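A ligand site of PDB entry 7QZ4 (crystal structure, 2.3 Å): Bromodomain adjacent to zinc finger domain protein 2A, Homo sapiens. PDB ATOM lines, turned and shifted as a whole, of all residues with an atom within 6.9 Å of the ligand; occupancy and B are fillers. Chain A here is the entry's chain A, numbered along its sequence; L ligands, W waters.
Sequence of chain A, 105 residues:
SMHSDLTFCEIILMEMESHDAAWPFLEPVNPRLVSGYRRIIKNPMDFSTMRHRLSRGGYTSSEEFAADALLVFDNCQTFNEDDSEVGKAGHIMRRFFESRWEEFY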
ATOM      1  N   TRP A  23      23.538  -3.633  21.078  1.00  0.00           N
ATOM      2  CA  TRP A  23      23.310  -2.945  22.341  1.00  0.00           C
ATOM      3  C   TRP A  23      23.658  -1.450  22.339  1.00  0.00           C
ATOM      4  O   TRP A  23      23.003  -0.715  23.091  1.00  0.00           O
ATOM      5  CB  TRP A  23      24.048  -3.684  23.459  1.00  0.00           C
ATOM      6  CG  TRP A  23      25.512  -3.764  23.216  1.00  0.00           C
ATOM      7  CD1 TRP A  23      26.179  -4.744  22.558  1.00  0.00           C
ATOM      8  CD2 TRP A  23      26.494  -2.798  23.617  1.00  0.00           C
ATOM      9  NE1 TRP A  23      27.522  -4.461  22.526  1.00  0.00           N
ATOM     10  CE2 TRP A  23      27.746  -3.272  23.162  1.00  0.00           C
ATOM     11  CE3 TRP A  23      26.443  -1.594  24.310  1.00  0.00           C
ATOM     12  CZ2 TRP A  23      28.935  -2.579  23.379  1.00  0.00           C
ATOM     13  CZ3 TRP A  23      27.623  -0.902  24.523  1.00  0.00           C
ATOM     14  CH2 TRP A  23      28.852  -1.401  24.070  1.00  0.00           C
ATOM     15  N   PRO A  24      24.630  -0.930  21.565  1.00  0.00           N
ATOM     16  CA  PRO A  24      24.862   0.524  21.573  1.00  0.00           C
ATOM     17  C   PRO A  24      23.794   1.329  20.890  1.00  0.00           C
ATOM     18  O   PRO A  24      23.714   2.542  21.126  1.00  0.00           O
ATOM     19  CB  PRO A  24      26.206   0.674  20.826  1.00  0.00           C
ATOM     20  CG  PRO A  24      26.824  -0.696  20.882  1.00  0.00           C
ATOM     21  CD  PRO A  24      25.665  -1.596  20.745  1.00  0.00           C
ATOM     22  N   PHE A  25      22.955   0.698  20.059  1.00  0.00           N
ATOM     23  CA  PHE A  25      22.125   1.428  19.104  1.00  0.00           C
ATOM     24  C   PHE A  25      20.636   1.255  19.337  1.00  0.00           C
ATOM     25  O   PHE A  25      19.845   1.712  18.513  1.00  0.00           O
ATOM     26  CB  PHE A  25      22.503   0.996  17.691  1.00  0.00           C
ATOM     27  CG  PHE A  25      23.972   0.938  17.482  1.00  0.00           C
ATOM     28  CD1 PHE A  25      24.705   2.093  17.302  1.00  0.00           C
ATOM     29  CD2 PHE A  25      24.647  -0.267  17.509  1.00  0.00           C
ATOM     30  CE1 PHE A  25      26.057   2.061  17.126  1.00  0.00           C
ATOM     31  CE2 PHE A  25      26.018  -0.309  17.339  1.00  0.00           C
ATOM     32  CZ  PHE A  25      26.720   0.874  17.153  1.00  0.00           C
ATOM     33  N   LEU A  26      20.227   0.623  20.442  1.00  0.00           N
ATOM     34  CA  LEU A  26      18.815   0.362  20.657  1.00  0.00           C
ATOM     35  C   LEU A  26      18.046   1.625  21.040  1.00  0.00           C
ATOM     36  O   LEU A  26      16.877   1.773  20.691  1.00  0.00           O
ATOM     37  CB  LEU A  26      18.635  -0.736  21.719  1.00  0.00           C
ATOM     38  CG  LEU A  26      19.305  -2.070  21.380  1.00  0.00           C
ATOM     39  CD1 LEU A  26      19.242  -2.994  22.562  1.00  0.00           C
ATOM     40  CD2 LEU A  26      18.669  -2.739  20.167  1.00  0.00           C
ATOM     41  N   GLU A  27      18.675   2.554  21.746  1.00  0.00           N
ATOM     42  CA  GLU A  27      18.032   3.790  22.145  1.00  0.00           C
ATOM     43  C   GLU A  27      18.948   4.957  21.801  1.00  0.00           C
ATOM     44  O   GLU A  27      20.151   4.768  21.613  1.00  0.00           O
ATOM     45  CB  GLU A  27      17.707   3.775  23.645  1.00  0.00           C
ATOM     46  CG  GLU A  27      18.391   2.710  24.477  1.00  0.00           C
ATOM     47  CD  GLU A  27      18.255   2.978  25.973  1.00  0.00           C
ATOM     48  OE1 GLU A  27      18.303   4.163  26.379  1.00  0.00           O
ATOM     49  OE2 GLU A  27      18.106   2.009  26.745  1.00  0.00           O
ATOM     50  N   PRO A  28      18.394   6.175  21.687  1.00  0.00           N
ATOM     51  CA  PRO A  28      19.239   7.335  21.328  1.00  0.00           C
ATOM     52  C   PRO A  28      20.331   7.550  22.357  1.00  0.00           C
ATOM     53  O   PRO A  28      20.157   7.270  23.541  1.00  0.00           O
ATOM     54  CB  PRO A  28      18.250   8.516  21.325  1.00  0.00           C
ATOM     55  CG  PRO A  28      16.887   7.906  21.275  1.00  0.00           C
ATOM     56  CD  PRO A  28      17.005   6.591  21.971  1.00  0.00           C
ATOM     57  N   VAL A  29      21.477   8.053  21.886  1.00  0.00           N
ATOM     58  CA  VAL A  29      22.539   8.418  22.813  1.00  0.00           C
ATOM     59  C   VAL A  29      22.026   9.542  23.717  1.00  0.00           C
ATOM     60  O   VAL A  29      21.394  10.489  23.255  1.00  0.00           O
ATOM     61  CB  VAL A  29      23.803   8.861  22.062  1.00  0.00           C
ATOM     62  CG1 VAL A  29      24.789   9.457  23.024  1.00  0.00           C
ATOM     63  CG2 VAL A  29      24.450   7.665  21.339  1.00  0.00           C
ATOM     64  N   LEU A  33      25.194  12.297  29.086  1.00  0.00           N
ATOM     65  CA  LEU A  33      26.136  11.305  29.579  1.00  0.00           C
ATOM     66  C   LEU A  33      27.364  11.161  28.692  1.00  0.00           C
ATOM     67  O   LEU A  33      28.306  10.456  29.067  1.00  0.00           O
ATOM     68  CB  LEU A  33      25.441   9.934  29.689  1.00  0.00           C
ATOM     69  CG  LEU A  33      24.153   9.916  30.523  1.00  0.00           C
ATOM     70  CD1 LEU A  33      23.408   8.579  30.375  1.00  0.00           C
ATOM     71  CD2 LEU A  33      24.448  10.199  31.980  1.00  0.00           C
ATOM     72  N   VAL A  34      27.380  11.801  27.524  1.00  0.00           N
ATOM     73  CA  VAL A  34      28.458  11.614  26.559  1.00  0.00           C
ATOM     74  C   VAL A  34      29.002  12.990  26.235  1.00  0.00           C
ATOM     75  O   VAL A  34      28.467  13.705  25.385  1.00  0.00           O
ATOM     76  CB  VAL A  34      27.987  10.882  25.286  1.00  0.00           C
ATOM     77  CG1 VAL A  34      29.137  10.758  24.286  1.00  0.00           C
ATOM     78  CG2 VAL A  34      27.431   9.487  25.633  1.00  0.00           C
ATOM     79  N   TYR A  37      28.939  14.893  22.506  1.00  0.00           N
ATOM     80  CA  TYR A  37      28.151  14.218  21.485  1.00  0.00           C
ATOM     81  C   TYR A  37      27.359  15.216  20.645  1.00  0.00           C
ATOM     82  O   TYR A  37      27.397  15.153  19.409  1.00  0.00           O
ATOM     83  CB  TYR A  37      27.209  13.191  22.101  1.00  0.00           C
ATOM     84  CG  TYR A  37      26.718  12.202  21.055  1.00  0.00           C
ATOM     85  CD1 TYR A  37      27.567  11.229  20.547  1.00  0.00           C
ATOM     86  CD2 TYR A  37      25.411  12.258  20.581  1.00  0.00           C
ATOM     87  CE1 TYR A  37      27.142  10.331  19.590  1.00  0.00           C
ATOM     88  CE2 TYR A  37      24.961  11.350  19.607  1.00  0.00           C
ATOM     89  CZ  TYR A  37      25.844  10.387  19.120  1.00  0.00           C
ATOM     90  OH  TYR A  37      25.457   9.476  18.154  1.00  0.00           O
ATOM     91  N   ILE A  41      27.860  15.285  16.578  1.00  0.00           N
ATOM     92  CA  ILE A  41      26.903  14.502  15.809  1.00  0.00           C
ATOM     93  C   ILE A  41      25.685  15.375  15.581  1.00  0.00           C
ATOM     94  O   ILE A  41      24.834  15.534  16.473  1.00  0.00           O
ATOM     95  CB  ILE A  41      26.535  13.196  16.538  1.00  0.00           C
ATOM     96  CG1 ILE A  41      27.726  12.257  16.577  1.00  0.00           C
ATOM     97  CG2 ILE A  41      25.320  12.545  15.901  1.00  0.00           C
ATOM     98  CD1 ILE A  41      28.283  11.972  15.224  1.00  0.00           C
ATOM     99  N   MET A  45      20.837   9.224  15.237  1.00  0.00           N
ATOM    100  CA  MET A  45      19.897   8.198  14.776  1.00  0.00           C
ATOM    101  C   MET A  45      20.165   6.901  15.530  1.00  0.00           C
ATOM    102  O   MET A  45      21.301   6.608  15.927  1.00  0.00           O
ATOM    103  CB  MET A  45      20.012   7.987  13.255  1.00  0.00           C
ATOM    104  CG  MET A  45      18.995   7.072  12.655  1.00  0.00           C
ATOM    105  SD  MET A  45      17.285   7.400  13.113  1.00  0.00           S
ATOM    106  CE  MET A  45      17.063   9.021  12.393  1.00  0.00           C
ATOM    107  N   VAL A  72      23.173   5.726  11.337  1.00  0.00           N
ATOM    108  CA  VAL A  72      23.552   5.155  12.631  1.00  0.00           C
ATOM    109  C   VAL A  72      25.041   4.845  12.658  1.00  0.00           C
ATOM    110  O   VAL A  72      25.758   5.223  13.607  1.00  0.00           O
ATOM    111  CB  VAL A  72      22.726   3.903  12.955  1.00  0.00           C
ATOM    112  CG1 VAL A  72      23.144   3.364  14.303  1.00  0.00           C
ATOM    113  CG2 VAL A  72      21.243   4.195  12.960  1.00  0.00           C
ATOM    114  N   ASN A  75      27.470   8.023  12.137  1.00  0.00           N
ATOM    115  CA  ASN A  75      27.627   8.677  13.436  1.00  0.00           C
ATOM    116  C   ASN A  75      28.531   7.874  14.355  1.00  0.00           C
ATOM    117  O   ASN A  75      29.355   8.437  15.084  1.00  0.00           O
ATOM    118  CB  ASN A  75      26.263   8.874  14.100  1.00  0.00           C
ATOM    119  CG  ASN A  75      25.392   9.853  13.355  1.00  0.00           C
ATOM    120  OD1 ASN A  75      25.860  10.548  12.465  1.00  0.00           O
ATOM    121  ND2 ASN A  75      24.117   9.895  13.689  1.00  0.00           N
ATOM    122  N   CYS A  76      28.394   6.544  14.334  1.00  0.00           N
ATOM    123  CA  CYS A  76      29.208   5.692  15.190  1.00  0.00           C
ATOM    124  C   CYS A  76      30.682   5.829  14.855  1.00  0.00           C
ATOM    125  O   CYS A  76      31.532   5.993  15.745  1.00  0.00           O
ATOM    126  CB  CYS A  76      28.747   4.244  15.036  1.00  0.00           C
ATOM    127  SG  CYS A  76      29.750   3.114  16.015  1.00  0.00           S
ATOM    128  N   PHE A  79      32.152   9.375  15.881  1.00  0.00           N
ATOM    129  CA  PHE A  79      32.408   9.721  17.282  1.00  0.00           C
ATOM    130  C   PHE A  79      33.324   8.754  18.007  1.00  0.00           C
ATOM    131  O   PHE A  79      34.046   9.186  18.919  1.00  0.00           O
ATOM    132  CB  PHE A  79      31.088   9.802  18.042  1.00  0.00           C
ATOM    133  CG  PHE A  79      31.227  10.475  19.376  1.00  0.00           C
ATOM    134  CD1 PHE A  79      31.092  11.860  19.494  1.00  0.00           C
ATOM    135  CD2 PHE A  79      31.513   9.736  20.504  1.00  0.00           C
ATOM    136  CE1 PHE A  79      31.243  12.478  20.695  1.00  0.00           C
ATOM    137  CE2 PHE A  79      31.653  10.357  21.725  1.00  0.00           C
ATOM    138  CZ  PHE A  79      31.515  11.736  21.828  1.00  0.00           C
ATOM    139  N   ASN A  80      33.296   7.456  17.675  1.00  0.00           N
ATOM    140  CA  ASN A  80      34.000   6.418  18.422  1.00  0.00           C
ATOM    141  C   ASN A  80      35.201   5.902  17.645  1.00  0.00           C
ATOM    142  O   ASN A  80      35.142   5.725  16.425  1.00  0.00           O
ATOM    143  CB  ASN A  80      33.073   5.241  18.722  1.00  0.00           C
ATOM    144  CG  ASN A  80      31.808   5.676  19.450  1.00  0.00           C
ATOM    145  OD1 ASN A  80      31.812   5.825  20.667  1.00  0.00           O
ATOM    146  ND2 ASN A  80      30.740   5.892  18.695  1.00  0.00           N
ATOM    147  N   SER A  84      37.415   1.101  19.887  1.00  0.00           N
ATOM    148  CA  SER A  84      36.588   1.239  21.088  1.00  0.00           C
ATOM    149  C   SER A  84      35.511   0.168  21.082  1.00  0.00           C
ATOM    150  O   SER A  84      35.154  -0.393  20.046  1.00  0.00           O
ATOM    151  CB  SER A  84      35.939   2.620  21.161  1.00  0.00           C
ATOM    152  OG  SER A  84      34.817   2.701  20.295  1.00  0.00           O
ATOM    153  N   GLU A  85      34.971  -0.090  22.282  1.00  0.00           N
ATOM    154  CA  GLU A  85      33.969  -1.137  22.416  1.00  0.00           C
ATOM    155  C   GLU A  85      32.702  -0.797  21.630  1.00  0.00           C
ATOM    156  O   GLU A  85      32.057  -1.701  21.090  1.00  0.00           O
ATOM    157  CB  GLU A  85      33.686  -1.364  23.906  1.00  0.00           C
ATOM    158  CG  GLU A  85      32.268  -1.814  24.227  1.00  0.00           C
ATOM    159  CD  GLU A  85      31.990  -1.895  25.725  1.00  0.00           C
ATOM    160  OE1 GLU A  85      32.202  -2.957  26.360  1.00  0.00           O
ATOM    161  OE2 GLU A  85      31.549  -0.873  26.287  1.00  0.00           O
ATOM    162  N   VAL A  86      32.359   0.495  21.518  1.00  0.00           N
ATOM    163  CA  VAL A  86      31.190   0.846  20.715  1.00  0.00           C
ATOM    164  C   VAL A  86      31.543   0.851  19.226  1.00  0.00           C
ATOM    165  O   VAL A  86      30.762   0.411  18.387  1.00  0.00           O
ATOM    166  CB  VAL A  86      30.605   2.206  21.153  1.00  0.00           C
ATOM    167  CG1 VAL A  86      29.682   2.758  20.075  1.00  0.00           C
ATOM    168  CG2 VAL A  86      29.863   2.069  22.484  1.00  0.00           C
HETATM  169  C1  LIG L   1      22.682   0.216  28.289  1.00  0.00           C
HETATM  170  C2  LIG L   1      25.211   2.075  26.108  1.00  0.00           C
HETATM  171  C3  LIG L   1      26.556   3.431  24.742  1.00  0.00           C
HETATM  172  C4  LIG L   1      26.808   4.252  23.475  1.00  0.00           C
HETATM  173  N1  LIG L   1      26.134   3.979  22.327  1.00  0.00           N
HETATM  174  C5  LIG L   1      26.525   4.804  21.342  1.00  0.00           C
HETATM  175  C6  LIG L   1      27.520   5.670  21.878  1.00  0.00           C
HETATM  176  C7  LIG L   1      28.219   6.772  21.051  1.00  0.00           C
HETATM  177  C8  LIG L   1      28.933   7.972  21.733  1.00  0.00           C
HETATM  178  C9  LIG L   1      28.645   5.878  24.316  1.00  0.00           C
HETATM  179  C10 LIG L   1      19.577  -1.736  29.929  1.00  0.00           C
HETATM  180  C11 LIG L   1      18.681  -2.952  29.608  1.00  0.00           C
HETATM  181  C12 LIG L   1      18.856  -6.216  30.495  1.00  0.00           C
HETATM  182  C13 LIG L   1      19.365  -4.764  30.663  1.00  0.00           C
HETATM  183  C14 LIG L   1      20.776  -4.121  29.142  1.00  0.00           C
HETATM  184  C15 LIG L   1      21.129  -2.828  28.377  1.00  0.00           C
HETATM  185  C16 LIG L   1      20.761  -1.592  29.077  1.00  0.00           C
HETATM  186  C17 LIG L   1      20.557  -0.380  27.995  1.00  0.00           C
HETATM  187  C18 LIG L   1      21.462   1.076  26.590  1.00  0.00           C
HETATM  188  C19 LIG L   1      22.717   1.628  25.897  1.00  0.00           C
HETATM  189  C20 LIG L   1      24.009   0.328  27.555  1.00  0.00           C
HETATM  190  C21 LIG L   1      27.470   3.088  25.786  1.00  0.00           C
HETATM  191  C22 LIG L   1      25.923   4.749  19.910  1.00  0.00           C
HETATM  192  C23 LIG L   1      27.697   5.312  23.232  1.00  0.00           C
HETATM  193  C24 LIG L   1      30.104   5.444  24.095  1.00  0.00           C
HETATM  194  N2  LIG L   1      19.409  -4.202  29.598  1.00  0.00           N
HETATM  195  N3  LIG L   1      21.679  -0.034  27.397  1.00  0.00           N
HETATM  196  N4  LIG L   1      24.001   1.375  26.534  1.00  0.00           N
HETATM  197  N5  LIG L   1      25.227   2.800  24.936  1.00  0.00           N
HETATM  198  O1  LIG L   1      28.201   6.740  19.858  1.00  0.00           O
HETATM  199  S1  LIG L   1      26.696   2.150  26.847  1.00  0.00           S
HETATM  200  O   HOH W   1      22.535   4.910  20.286  1.00  0.00           O
HETATM  201  O   HOH W   2      27.108   7.590  17.748  1.00  0.00           O
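An oxygen (O1) of the ligand is in hydrogen-bond range of the side-chain amide nitrogen (ND2) of Asn 80 (2.9 Å).
The backbone carbonyl oxygen of Pro 24 lies within hydrogen-bond range of a nitrogen (N1) of the ligand.
The side-chain sulfur (SG) of Cys 76 is in hydrogen-bond range of the backbone carbonyl oxygen (O) of Val 86, at 3.7 Å.
O of Cys 76 is in hydrogen-bond range of ND2 of Asn 80 (3.1 Å).
Residues that only touch the ligand: Phe 79 (3.4 Å), Glu 27 (3.5 Å), Val 29 (3.5 Å), Tyr 37 (3.7 Å), Trp 23 (3.7 Å), Val 86 (3.7 Å), Val 34 (3.8 Å) and Phe 25 (3.9 Å).
Hydrophobic or aromatic side chains that line the ligand: Trp 23, Pro 24, Phe 25, Val 29, Val 34, Tyr 37, Phe 79 and Val 86.
Of the 20 residues printed, 10 come within 4 Å of the ligand.
Water W2 lies within hydrogen-bond range of O1 of the ligand (2.5 Å) and OH of Tyr 37 (2.5 Å).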
